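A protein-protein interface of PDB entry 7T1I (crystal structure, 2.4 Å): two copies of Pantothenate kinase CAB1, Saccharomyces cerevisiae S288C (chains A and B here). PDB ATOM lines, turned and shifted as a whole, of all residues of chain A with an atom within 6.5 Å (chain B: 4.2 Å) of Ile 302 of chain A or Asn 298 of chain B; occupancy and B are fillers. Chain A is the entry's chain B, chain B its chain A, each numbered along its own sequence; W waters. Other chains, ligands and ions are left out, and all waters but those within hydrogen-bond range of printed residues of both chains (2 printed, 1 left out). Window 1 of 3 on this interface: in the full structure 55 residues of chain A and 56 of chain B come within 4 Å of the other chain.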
ATOM      1  N   LEU A 160     -16.528  10.613 -13.086  1.00  0.00           N
ATOM      2  CA  LEU A 160     -15.845   9.426 -12.613  1.00  0.00           C
ATOM      3  C   LEU A 160     -15.644   8.440 -13.763  1.00  0.00           C
ATOM      4  O   LEU A 160     -16.439   8.376 -14.710  1.00  0.00           O
ATOM      5  CB  LEU A 160     -16.702   8.804 -11.508  1.00  0.00           C
ATOM      6  CG  LEU A 160     -15.932   7.945 -10.497  1.00  0.00           C
ATOM      7  CD1 LEU A 160     -15.170   8.842  -9.523  1.00  0.00           C
ATOM      8  CD2 LEU A 160     -16.856   7.011  -9.735  1.00  0.00           C
ATOM      9  N   VAL A 162     -14.885   4.298 -14.025  1.00  0.00           N
ATOM     10  CA  VAL A 162     -14.737   3.005 -13.405  1.00  0.00           C
ATOM     11  C   VAL A 162     -14.231   2.102 -14.525  1.00  0.00           C
ATOM     12  O   VAL A 162     -14.948   1.851 -15.497  1.00  0.00           O
ATOM     13  CB  VAL A 162     -16.067   2.521 -12.773  1.00  0.00           C
ATOM     14  CG1 VAL A 162     -15.976   1.092 -12.253  1.00  0.00           C
ATOM     15  CG2 VAL A 162     -16.534   3.475 -11.677  1.00  0.00           C
ATOM     16  N   VAL A 168     -10.337  -3.508 -10.933  1.00  0.00           N
ATOM     17  CA  VAL A 168     -11.011  -2.240 -11.128  1.00  0.00           C
ATOM     18  C   VAL A 168     -10.144  -1.111 -10.599  1.00  0.00           C
ATOM     19  O   VAL A 168      -9.686  -1.140  -9.446  1.00  0.00           O
ATOM     20  CB  VAL A 168     -12.386  -2.224 -10.435  1.00  0.00           C
ATOM     21  CG1 VAL A 168     -13.119  -0.920 -10.700  1.00  0.00           C
ATOM     22  CG2 VAL A 168     -13.248  -3.437 -10.789  1.00  0.00           C
ATOM     23  N   ILE A 170     -10.598   3.197 -10.204  1.00  0.00           N
ATOM     24  CA  ILE A 170     -11.548   4.296 -10.213  1.00  0.00           C
ATOM     25  C   ILE A 170     -10.794   5.620 -10.252  1.00  0.00           C
ATOM     26  O   ILE A 170      -9.861   5.826  -9.468  1.00  0.00           O
ATOM     27  CB  ILE A 170     -12.504   4.214  -9.008  1.00  0.00           C
ATOM     28  CG1 ILE A 170     -13.217   2.857  -9.027  1.00  0.00           C
ATOM     29  CG2 ILE A 170     -13.489   5.391  -9.043  1.00  0.00           C
ATOM     30  CD1 ILE A 170     -14.318   2.708  -8.029  1.00  0.00           C
ATOM     31  N   GLY A 184      -9.615   1.601  -6.199  1.00  0.00           N
ATOM     32  CA  GLY A 184      -9.662   0.437  -7.076  1.00  0.00           C
ATOM     33  C   GLY A 184     -10.180  -0.782  -6.320  1.00  0.00           C
ATOM     34  O   GLY A 184     -10.395  -0.723  -5.112  1.00  0.00           O
ATOM     35  N   SER A 185     -10.385  -1.882  -7.044  1.00  0.00           N
ATOM     36  CA  SER A 185     -10.931  -3.080  -6.444  1.00  0.00           C
ATOM     37  C   SER A 185     -10.371  -4.315  -7.140  1.00  0.00           C
ATOM     38  O   SER A 185     -10.316  -4.373  -8.378  1.00  0.00           O
ATOM     39  CB  SER A 185     -12.433  -3.083  -6.503  1.00  0.00           C
ATOM     40  OG  SER A 185     -12.963  -4.245  -5.851  1.00  0.00           O
ATOM     41  N   SER A 186     -10.013  -5.312  -6.322  1.00  0.00           N
ATOM     42  CA  SER A 186      -9.526  -6.579  -6.842  1.00  0.00           C
ATOM     43  C   SER A 186     -10.682  -7.467  -7.304  1.00  0.00           C
ATOM     44  O   SER A 186     -10.453  -8.558  -7.808  1.00  0.00           O
ATOM     45  CB  SER A 186      -8.662  -7.286  -5.821  1.00  0.00           C
ATOM     46  OG  SER A 186      -9.486  -7.948  -4.862  1.00  0.00           O
ATOM     47  N   LEU A 187     -11.926  -7.031  -7.085  1.00  0.00           N
ATOM     48  CA  LEU A 187     -13.064  -7.857  -7.470  1.00  0.00           C
ATOM     49  C   LEU A 187     -13.566  -7.391  -8.833  1.00  0.00           C
ATOM     50  O   LEU A 187     -14.489  -6.600  -8.899  1.00  0.00           O
ATOM     51  CB  LEU A 187     -14.160  -7.768  -6.397  1.00  0.00           C
ATOM     52  CG  LEU A 187     -13.753  -8.316  -5.029  1.00  0.00           C
ATOM     53  CD1 LEU A 187     -14.818  -7.997  -3.989  1.00  0.00           C
ATOM     54  CD2 LEU A 187     -13.505  -9.816  -5.110  1.00  0.00           C
ATOM     55  N   ASN A 297     -22.919  -5.463  -8.640  1.00  0.00           N
ATOM     56  CA  ASN A 297     -23.481  -4.624  -7.585  1.00  0.00           C
ATOM     57  C   ASN A 297     -22.355  -4.042  -6.727  1.00  0.00           C
ATOM     58  O   ASN A 297     -22.432  -2.911  -6.262  1.00  0.00           O
ATOM     59  CB  ASN A 297     -24.543  -5.336  -6.727  1.00  0.00           C
ATOM     60  CG  ASN A 297     -25.870  -5.626  -7.414  1.00  0.00           C
ATOM     61  OD1 ASN A 297     -26.257  -5.004  -8.409  1.00  0.00           O
ATOM     62  ND2 ASN A 297     -26.596  -6.588  -6.878  1.00  0.00           N
ATOM     63  N   ASN A 298     -21.291  -4.811  -6.513  1.00  0.00           N
ATOM     64  CA  ASN A 298     -20.228  -4.314  -5.659  1.00  0.00           C
ATOM     65  C   ASN A 298     -19.569  -3.112  -6.338  1.00  0.00           C
ATOM     66  O   ASN A 298     -19.478  -2.027  -5.764  1.00  0.00           O
ATOM     67  CB  ASN A 298     -19.250  -5.433  -5.331  1.00  0.00           C
ATOM     68  CG  ASN A 298     -18.302  -5.084  -4.207  1.00  0.00           C
ATOM     69  OD1 ASN A 298     -18.744  -4.832  -3.088  1.00  0.00           O
ATOM     70  ND2 ASN A 298     -16.998  -5.119  -4.468  1.00  0.00           N
ATOM     71  N   ILE A 299     -19.100  -3.330  -7.577  1.00  0.00           N
ATOM     72  CA  ILE A 299     -18.573  -2.288  -8.450  1.00  0.00           C
ATOM     73  C   ILE A 299     -19.518  -1.085  -8.443  1.00  0.00           C
ATOM     74  O   ILE A 299     -19.075   0.047  -8.230  1.00  0.00           O
ATOM     75  CB  ILE A 299     -18.346  -2.839  -9.876  1.00  0.00           C
ATOM     76  CG1 ILE A 299     -17.196  -3.847  -9.895  1.00  0.00           C
ATOM     77  CG2 ILE A 299     -18.185  -1.718 -10.892  1.00  0.00           C
ATOM     78  CD1 ILE A 299     -17.196  -4.768 -11.087  1.00  0.00           C
ATOM     79  N   GLY A 300     -20.814  -1.346  -8.642  1.00  0.00           N
ATOM     80  CA  GLY A 300     -21.816  -0.302  -8.601  1.00  0.00           C
ATOM     81  C   GLY A 300     -21.716   0.535  -7.322  1.00  0.00           C
ATOM     82  O   GLY A 300     -21.666   1.762  -7.370  1.00  0.00           O
ATOM     83  N   GLN A 301     -21.697  -0.141  -6.172  1.00  0.00           N
ATOM     84  CA  GLN A 301     -21.719   0.483  -4.862  1.00  0.00           C
ATOM     85  C   GLN A 301     -20.465   1.322  -4.674  1.00  0.00           C
ATOM     86  O   GLN A 301     -20.506   2.455  -4.208  1.00  0.00           O
ATOM     87  CB  GLN A 301     -21.765  -0.595  -3.770  1.00  0.00           C
ATOM     88  CG  GLN A 301     -21.577   0.019  -2.383  1.00  0.00           C
ATOM     89  CD  GLN A 301     -21.699  -0.907  -1.194  1.00  0.00           C
ATOM     90  OE1 GLN A 301     -22.165  -2.047  -1.280  1.00  0.00           O
ATOM     91  NE2 GLN A 301     -21.246  -0.411  -0.057  1.00  0.00           N
ATOM     92  N   ILE A 302     -19.325   0.735  -5.023  1.00  0.00           N
ATOM     93  CA  ILE A 302     -18.078   1.440  -4.824  1.00  0.00           C
ATOM     94  C   ILE A 302     -18.002   2.658  -5.749  1.00  0.00           C
ATOM     95  O   ILE A 302     -17.514   3.717  -5.332  1.00  0.00           O
ATOM     96  CB  ILE A 302     -16.896   0.488  -5.003  1.00  0.00           C
ATOM     97  CG1 ILE A 302     -16.800  -0.508  -3.839  1.00  0.00           C
ATOM     98  CG2 ILE A 302     -15.621   1.288  -5.158  1.00  0.00           C
ATOM     99  CD1 ILE A 302     -15.723  -1.583  -4.036  1.00  0.00           C
ATOM    100  N   ALA A 303     -18.493   2.515  -6.986  1.00  0.00           N
ATOM    101  CA  ALA A 303     -18.562   3.638  -7.896  1.00  0.00           C
ATOM    102  C   ALA A 303     -19.445   4.725  -7.276  1.00  0.00           C
ATOM    103  O   ALA A 303     -19.114   5.905  -7.313  1.00  0.00           O
ATOM    104  CB  ALA A 303     -19.088   3.169  -9.233  1.00  0.00           C
ATOM    105  N   TYR A 304     -20.578   4.328  -6.686  1.00  0.00           N
ATOM    106  CA  TYR A 304     -21.476   5.300  -6.093  1.00  0.00           C
ATOM    107  C   TYR A 304     -20.724   6.026  -4.972  1.00  0.00           C
ATOM    108  O   TYR A 304     -20.672   7.257  -4.933  1.00  0.00           O
ATOM    109  CB  TYR A 304     -22.824   4.690  -5.674  1.00  0.00           C
ATOM    110  CG  TYR A 304     -23.599   5.602  -4.748  1.00  0.00           C
ATOM    111  CD1 TYR A 304     -24.369   6.650  -5.238  1.00  0.00           C
ATOM    112  CD2 TYR A 304     -23.519   5.459  -3.366  1.00  0.00           C
ATOM    113  CE1 TYR A 304     -25.050   7.512  -4.389  1.00  0.00           C
ATOM    114  CE2 TYR A 304     -24.216   6.278  -2.498  1.00  0.00           C
ATOM    115  CZ  TYR A 304     -24.957   7.328  -3.018  1.00  0.00           C
ATOM    116  OH  TYR A 304     -25.598   8.192  -2.186  1.00  0.00           O
ATOM    117  N   LEU A 305     -20.090   5.251  -4.098  1.00  0.00           N
ATOM    118  CA  LEU A 305     -19.501   5.864  -2.916  1.00  0.00           C
ATOM    119  C   LEU A 305     -18.420   6.863  -3.319  1.00  0.00           C
ATOM    120  O   LEU A 305     -18.391   7.971  -2.779  1.00  0.00           O
ATOM    121  CB  LEU A 305     -18.976   4.785  -1.963  1.00  0.00           C
ATOM    122  CG  LEU A 305     -20.071   3.883  -1.390  1.00  0.00           C
ATOM    123  CD1 LEU A 305     -19.486   2.807  -0.485  1.00  0.00           C
ATOM    124  CD2 LEU A 305     -21.119   4.718  -0.647  1.00  0.00           C
ATOM    125  N   GLN A 306     -17.593   6.476  -4.310  1.00  0.00           N
ATOM    126  CA  GLN A 306     -16.521   7.325  -4.806  1.00  0.00           C
ATOM    127  C   GLN A 306     -17.118   8.565  -5.455  1.00  0.00           C
ATOM    128  O   GLN A 306     -16.670   9.676  -5.166  1.00  0.00           O
ATOM    129  CB  GLN A 306     -15.556   6.619  -5.747  1.00  0.00           C
ATOM    130  CG  GLN A 306     -14.653   5.595  -5.054  1.00  0.00           C
ATOM    131  CD  GLN A 306     -13.512   6.136  -4.224  1.00  0.00           C
ATOM    132  OE1 GLN A 306     -13.531   7.269  -3.722  1.00  0.00           O
ATOM    133  NE2 GLN A 306     -12.503   5.291  -4.053  1.00  0.00           N
ATOM    134  N   ALA A 307     -18.164   8.372  -6.274  1.00  0.00           N
ATOM    135  CA  ALA A 307     -18.809   9.517  -6.895  1.00  0.00           C
ATOM    136  C   ALA A 307     -19.354  10.448  -5.817  1.00  0.00           C
ATOM    137  O   ALA A 307     -19.339  11.668  -5.990  1.00  0.00           O
ATOM    138  CB  ALA A 307     -19.900   9.066  -7.822  1.00  0.00           C
ATOM    139  N   LEU B 187     -21.600  -9.014  -0.076  1.00  0.00           N
ATOM    140  CA  LEU B 187     -20.351  -9.770  -0.033  1.00  0.00           C
ATOM    141  C   LEU B 187     -19.840  -9.833   1.414  1.00  0.00           C
ATOM    142  O   LEU B 187     -19.065  -8.978   1.849  1.00  0.00           O
ATOM    143  CB  LEU B 187     -19.316  -9.151  -0.990  1.00  0.00           C
ATOM    144  CG  LEU B 187     -19.731  -8.978  -2.455  1.00  0.00           C
ATOM    145  CD1 LEU B 187     -18.560  -8.487  -3.310  1.00  0.00           C
ATOM    146  CD2 LEU B 187     -20.267 -10.280  -3.027  1.00  0.00           C
ATOM    147  N   ALA B 294      -9.865 -11.248  -0.674  1.00  0.00           N
ATOM    148  CA  ALA B 294     -10.828 -10.590  -1.546  1.00  0.00           C
ATOM    149  C   ALA B 294     -11.977  -9.981  -0.733  1.00  0.00           C
ATOM    150  O   ALA B 294     -12.308  -8.803  -0.889  1.00  0.00           O
ATOM    151  CB  ALA B 294     -11.338 -11.551  -2.586  1.00  0.00           C
ATOM    152  N   ILE B 295     -12.575 -10.786   0.154  1.00  0.00           N
ATOM    153  CA  ILE B 295     -13.776 -10.341   0.838  1.00  0.00           C
ATOM    154  C   ILE B 295     -13.397  -9.324   1.908  1.00  0.00           C
ATOM    155  O   ILE B 295     -14.045  -8.293   2.023  1.00  0.00           O
ATOM    156  CB  ILE B 295     -14.608 -11.522   1.386  1.00  0.00           C
ATOM    157  CG1 ILE B 295     -14.963 -12.542   0.293  1.00  0.00           C
ATOM    158  CG2 ILE B 295     -15.853 -11.017   2.091  1.00  0.00           C
ATOM    159  CD1 ILE B 295     -15.789 -11.998  -0.857  1.00  0.00           C
ATOM    160  N   SER B 296     -12.311  -9.597   2.639  1.00  0.00           N
ATOM    161  CA  SER B 296     -11.894  -8.717   3.722  1.00  0.00           C
ATOM    162  C   SER B 296     -11.496  -7.347   3.198  1.00  0.00           C
ATOM    163  O   SER B 296     -11.794  -6.314   3.824  1.00  0.00           O
ATOM    164  CB  SER B 296     -10.784  -9.311   4.549  1.00  0.00           C
ATOM    165  OG  SER B 296     -11.221 -10.553   5.076  1.00  0.00           O
ATOM    166  N   ASN B 297     -10.773  -7.380   2.074  1.00  0.00           N
ATOM    167  CA  ASN B 297     -10.256  -6.151   1.508  1.00  0.00           C
ATOM    168  C   ASN B 297     -11.433  -5.316   1.017  1.00  0.00           C
ATOM    169  O   ASN B 297     -11.434  -4.095   1.190  1.00  0.00           O
ATOM    170  CB  ASN B 297      -9.227  -6.402   0.408  1.00  0.00           C
ATOM    171  CG  ASN B 297      -7.835  -6.756   0.903  1.00  0.00           C
ATOM    172  OD1 ASN B 297      -7.478  -6.546   2.067  1.00  0.00           O
ATOM    173  ND2 ASN B 297      -7.030  -7.297   0.008  1.00  0.00           N
ATOM    174  N   ASN B 298     -12.436  -5.998   0.452  1.00  0.00           N
ATOM    175  CA  ASN B 298     -13.608  -5.323  -0.060  1.00  0.00           C
ATOM    176  C   ASN B 298     -14.341  -4.655   1.101  1.00  0.00           C
ATOM    177  O   ASN B 298     -14.674  -3.470   1.005  1.00  0.00           O
ATOM    178  CB  ASN B 298     -14.554  -6.255  -0.822  1.00  0.00           C
ATOM    179  CG  ASN B 298     -15.564  -5.476  -1.637  1.00  0.00           C
ATOM    180  OD1 ASN B 298     -15.195  -4.727  -2.541  1.00  0.00           O
ATOM    181  ND2 ASN B 298     -16.842  -5.629  -1.343  1.00  0.00           N
ATOM    182  N   ILE B 299     -14.565  -5.415   2.194  1.00  0.00           N
ATOM    183  CA  ILE B 299     -15.221  -4.880   3.391  1.00  0.00           C
ATOM    184  C   ILE B 299     -14.423  -3.697   3.933  1.00  0.00           C
ATOM    185  O   ILE B 299     -14.983  -2.635   4.233  1.00  0.00           O
ATOM    186  CB  ILE B 299     -15.467  -5.974   4.454  1.00  0.00           C
ATOM    187  CG1 ILE B 299     -16.485  -7.004   3.945  1.00  0.00           C
ATOM    188  CG2 ILE B 299     -15.861  -5.371   5.811  1.00  0.00           C
ATOM    189  CD1 ILE B 299     -16.472  -8.327   4.699  1.00  0.00           C
ATOM    190  N   GLY B 300     -13.106  -3.899   4.009  1.00  0.00           N
ATOM    191  CA  GLY B 300     -12.210  -2.838   4.415  1.00  0.00           C
ATOM    192  C   GLY B 300     -12.450  -1.560   3.616  1.00  0.00           C
ATOM    193  O   GLY B 300     -12.646  -0.505   4.214  1.00  0.00           O
ATOM    194  N   GLN B 301     -12.453  -1.669   2.274  1.00  0.00           N
ATOM    195  CA  GLN B 301     -12.616  -0.509   1.408  1.00  0.00           C
ATOM    196  C   GLN B 301     -13.976   0.153   1.638  1.00  0.00           C
ATOM    197  O   GLN B 301     -14.085   1.364   1.773  1.00  0.00           O
ATOM    198  CB  GLN B 301     -12.426  -0.887  -0.059  1.00  0.00           C
ATOM    199  CG  GLN B 301     -12.802   0.252  -1.005  1.00  0.00           C
ATOM    200  CD  GLN B 301     -12.604  -0.063  -2.475  1.00  0.00           C
ATOM    201  OE1 GLN B 301     -12.076  -1.116  -2.854  1.00  0.00           O
ATOM    202  NE2 GLN B 301     -13.083   0.835  -3.322  1.00  0.00           N
ATOM    203  N   ILE B 302     -15.044  -0.636   1.700  1.00  0.00           N
ATOM    204  CA  ILE B 302     -16.342  -0.006   1.857  1.00  0.00           C
ATOM    205  C   ILE B 302     -16.440   0.687   3.225  1.00  0.00           C
ATOM    206  O   ILE B 302     -16.931   1.822   3.302  1.00  0.00           O
ATOM    207  CB  ILE B 302     -17.477  -0.997   1.568  1.00  0.00           C
ATOM    208  CG1 ILE B 302     -17.522  -1.342   0.074  1.00  0.00           C
ATOM    209  CG2 ILE B 302     -18.810  -0.476   2.086  1.00  0.00           C
ATOM    210  CD1 ILE B 302     -18.333  -2.599  -0.254  1.00  0.00           C
HETATM  211  O   HOH W   1     -11.237  -6.711  -2.654  1.00  0.00           O
HETATM  212  O   HOH W   2     -12.761  -4.750  -3.339  1.00  0.00           O
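Of the 19 printed residues of chain A, 5 touch a printed residue of chain B. Along chain A the printed residues that touch a printed residue of chain B span positions 184 to 302. Among the printed residues, 10 pairs touch across the chains. Among the printed residues, no Asp or Glu carboxylate lies within 4 Å of a Lys or Arg side-chain nitrogen of the other chain.
Water W2 bridges the side-chain amide oxygen (OD1) of Asn 298 of chain B (2.6 Å) and the side-chain hydroxyl (OG) of Ser 185 of chain A (2.6 Å). Water W1 lies within hydrogen-bond range of O of Ala 294 of chain B, OG of Ser 186 of chain A and N of Asn 298 of chain B.
Leu 187 of chain A touches Asn 298 of chain B, and with the chains exchanged Asn 298 of chain A touches Leu 187 of chain B. Asn 298 of chain A touches its own counterpart, Asn 298 of chain B. Asn 298 of chain A touches Ile 302 of chain B, and with the chains exchanged Ile 302 of chain A touches Asn 298 of chain B. Gln 301 of chain A touches Ile 302 of chain B, and with the chains exchanged Ile 302 of chain A touches Gln 301 of chain B. Positions printed for both chains: 187, 297, 298, 299, 300, 301 and 302. Of the 10 pairs that touch across the chains among the printed residues, 8 have their exchanged pair printed and touching as well.
Among the printed residues, merely in contact across the chains: Leu 187 of chain A with Leu 187 of chain B (3.8 Å), Leu 187 of chain A with Ala 294 of chain B (3.8 Å), Leu 187 of chain A with Asn 298 of chain B (3.5 Å), Asn 298 of chain A with Leu 187 of chain B (3.5 Å), Asn 298 of chain A with Ile 302 of chain B (3.6 Å), Gln 301 of chain A with Ile 302 of chain B (3.2 Å), Ile 302 of chain A with Asn 298 of chain B (3.5 Å) and Ile 302 of chain A with Gln 301 of chain B (3.2 Å).
The backbone NH of Leu 187 of chain A lies close to the side-chain hydroxyl of Ser 185 of chain A (3.2 Å).
ND2 of Asn 298 of chain A lies within hydrogen-bond range of OD1 of Asn 298 of chain B. O of Gly 184 of chain A lies close to OE1 of Gln 301 of chain B, 2.8 Å away.
Of the printed residues of chain B, Gly 184 of chain A touches Gln 301 (2.8 Å). Of the printed residues of chain B, Leu 187 of chain A touches Leu 187 (3.8 Å), Ala 294 (3.8 Å) and Asn 298 (3.5 Å). Of the printed residues of chain B, Asn 298 of chain A touches Leu 187 (3.5 Å), Asn 298 (2.7 Å) and Ile 302 (3.6 Å). Printed residues of chain A within 4 Å of Ala 294 of chain B: Leu 187. Ser 296 of chain B touches none of the printed residues of chain A. Asn 298 of chain B touches three residues of chain A. Printed residues of chain A within 4 Å of Ile 302 of chain B: Asn 298 and Gln 301. The nearest residue of chain B that does not touch Ile 302 of chain A is Ile 302 of chain B (4.1 Å). The nearest residue of chain A that does not touch Asn 298 of chain B is Ser 185 of chain A (4.02 Å).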
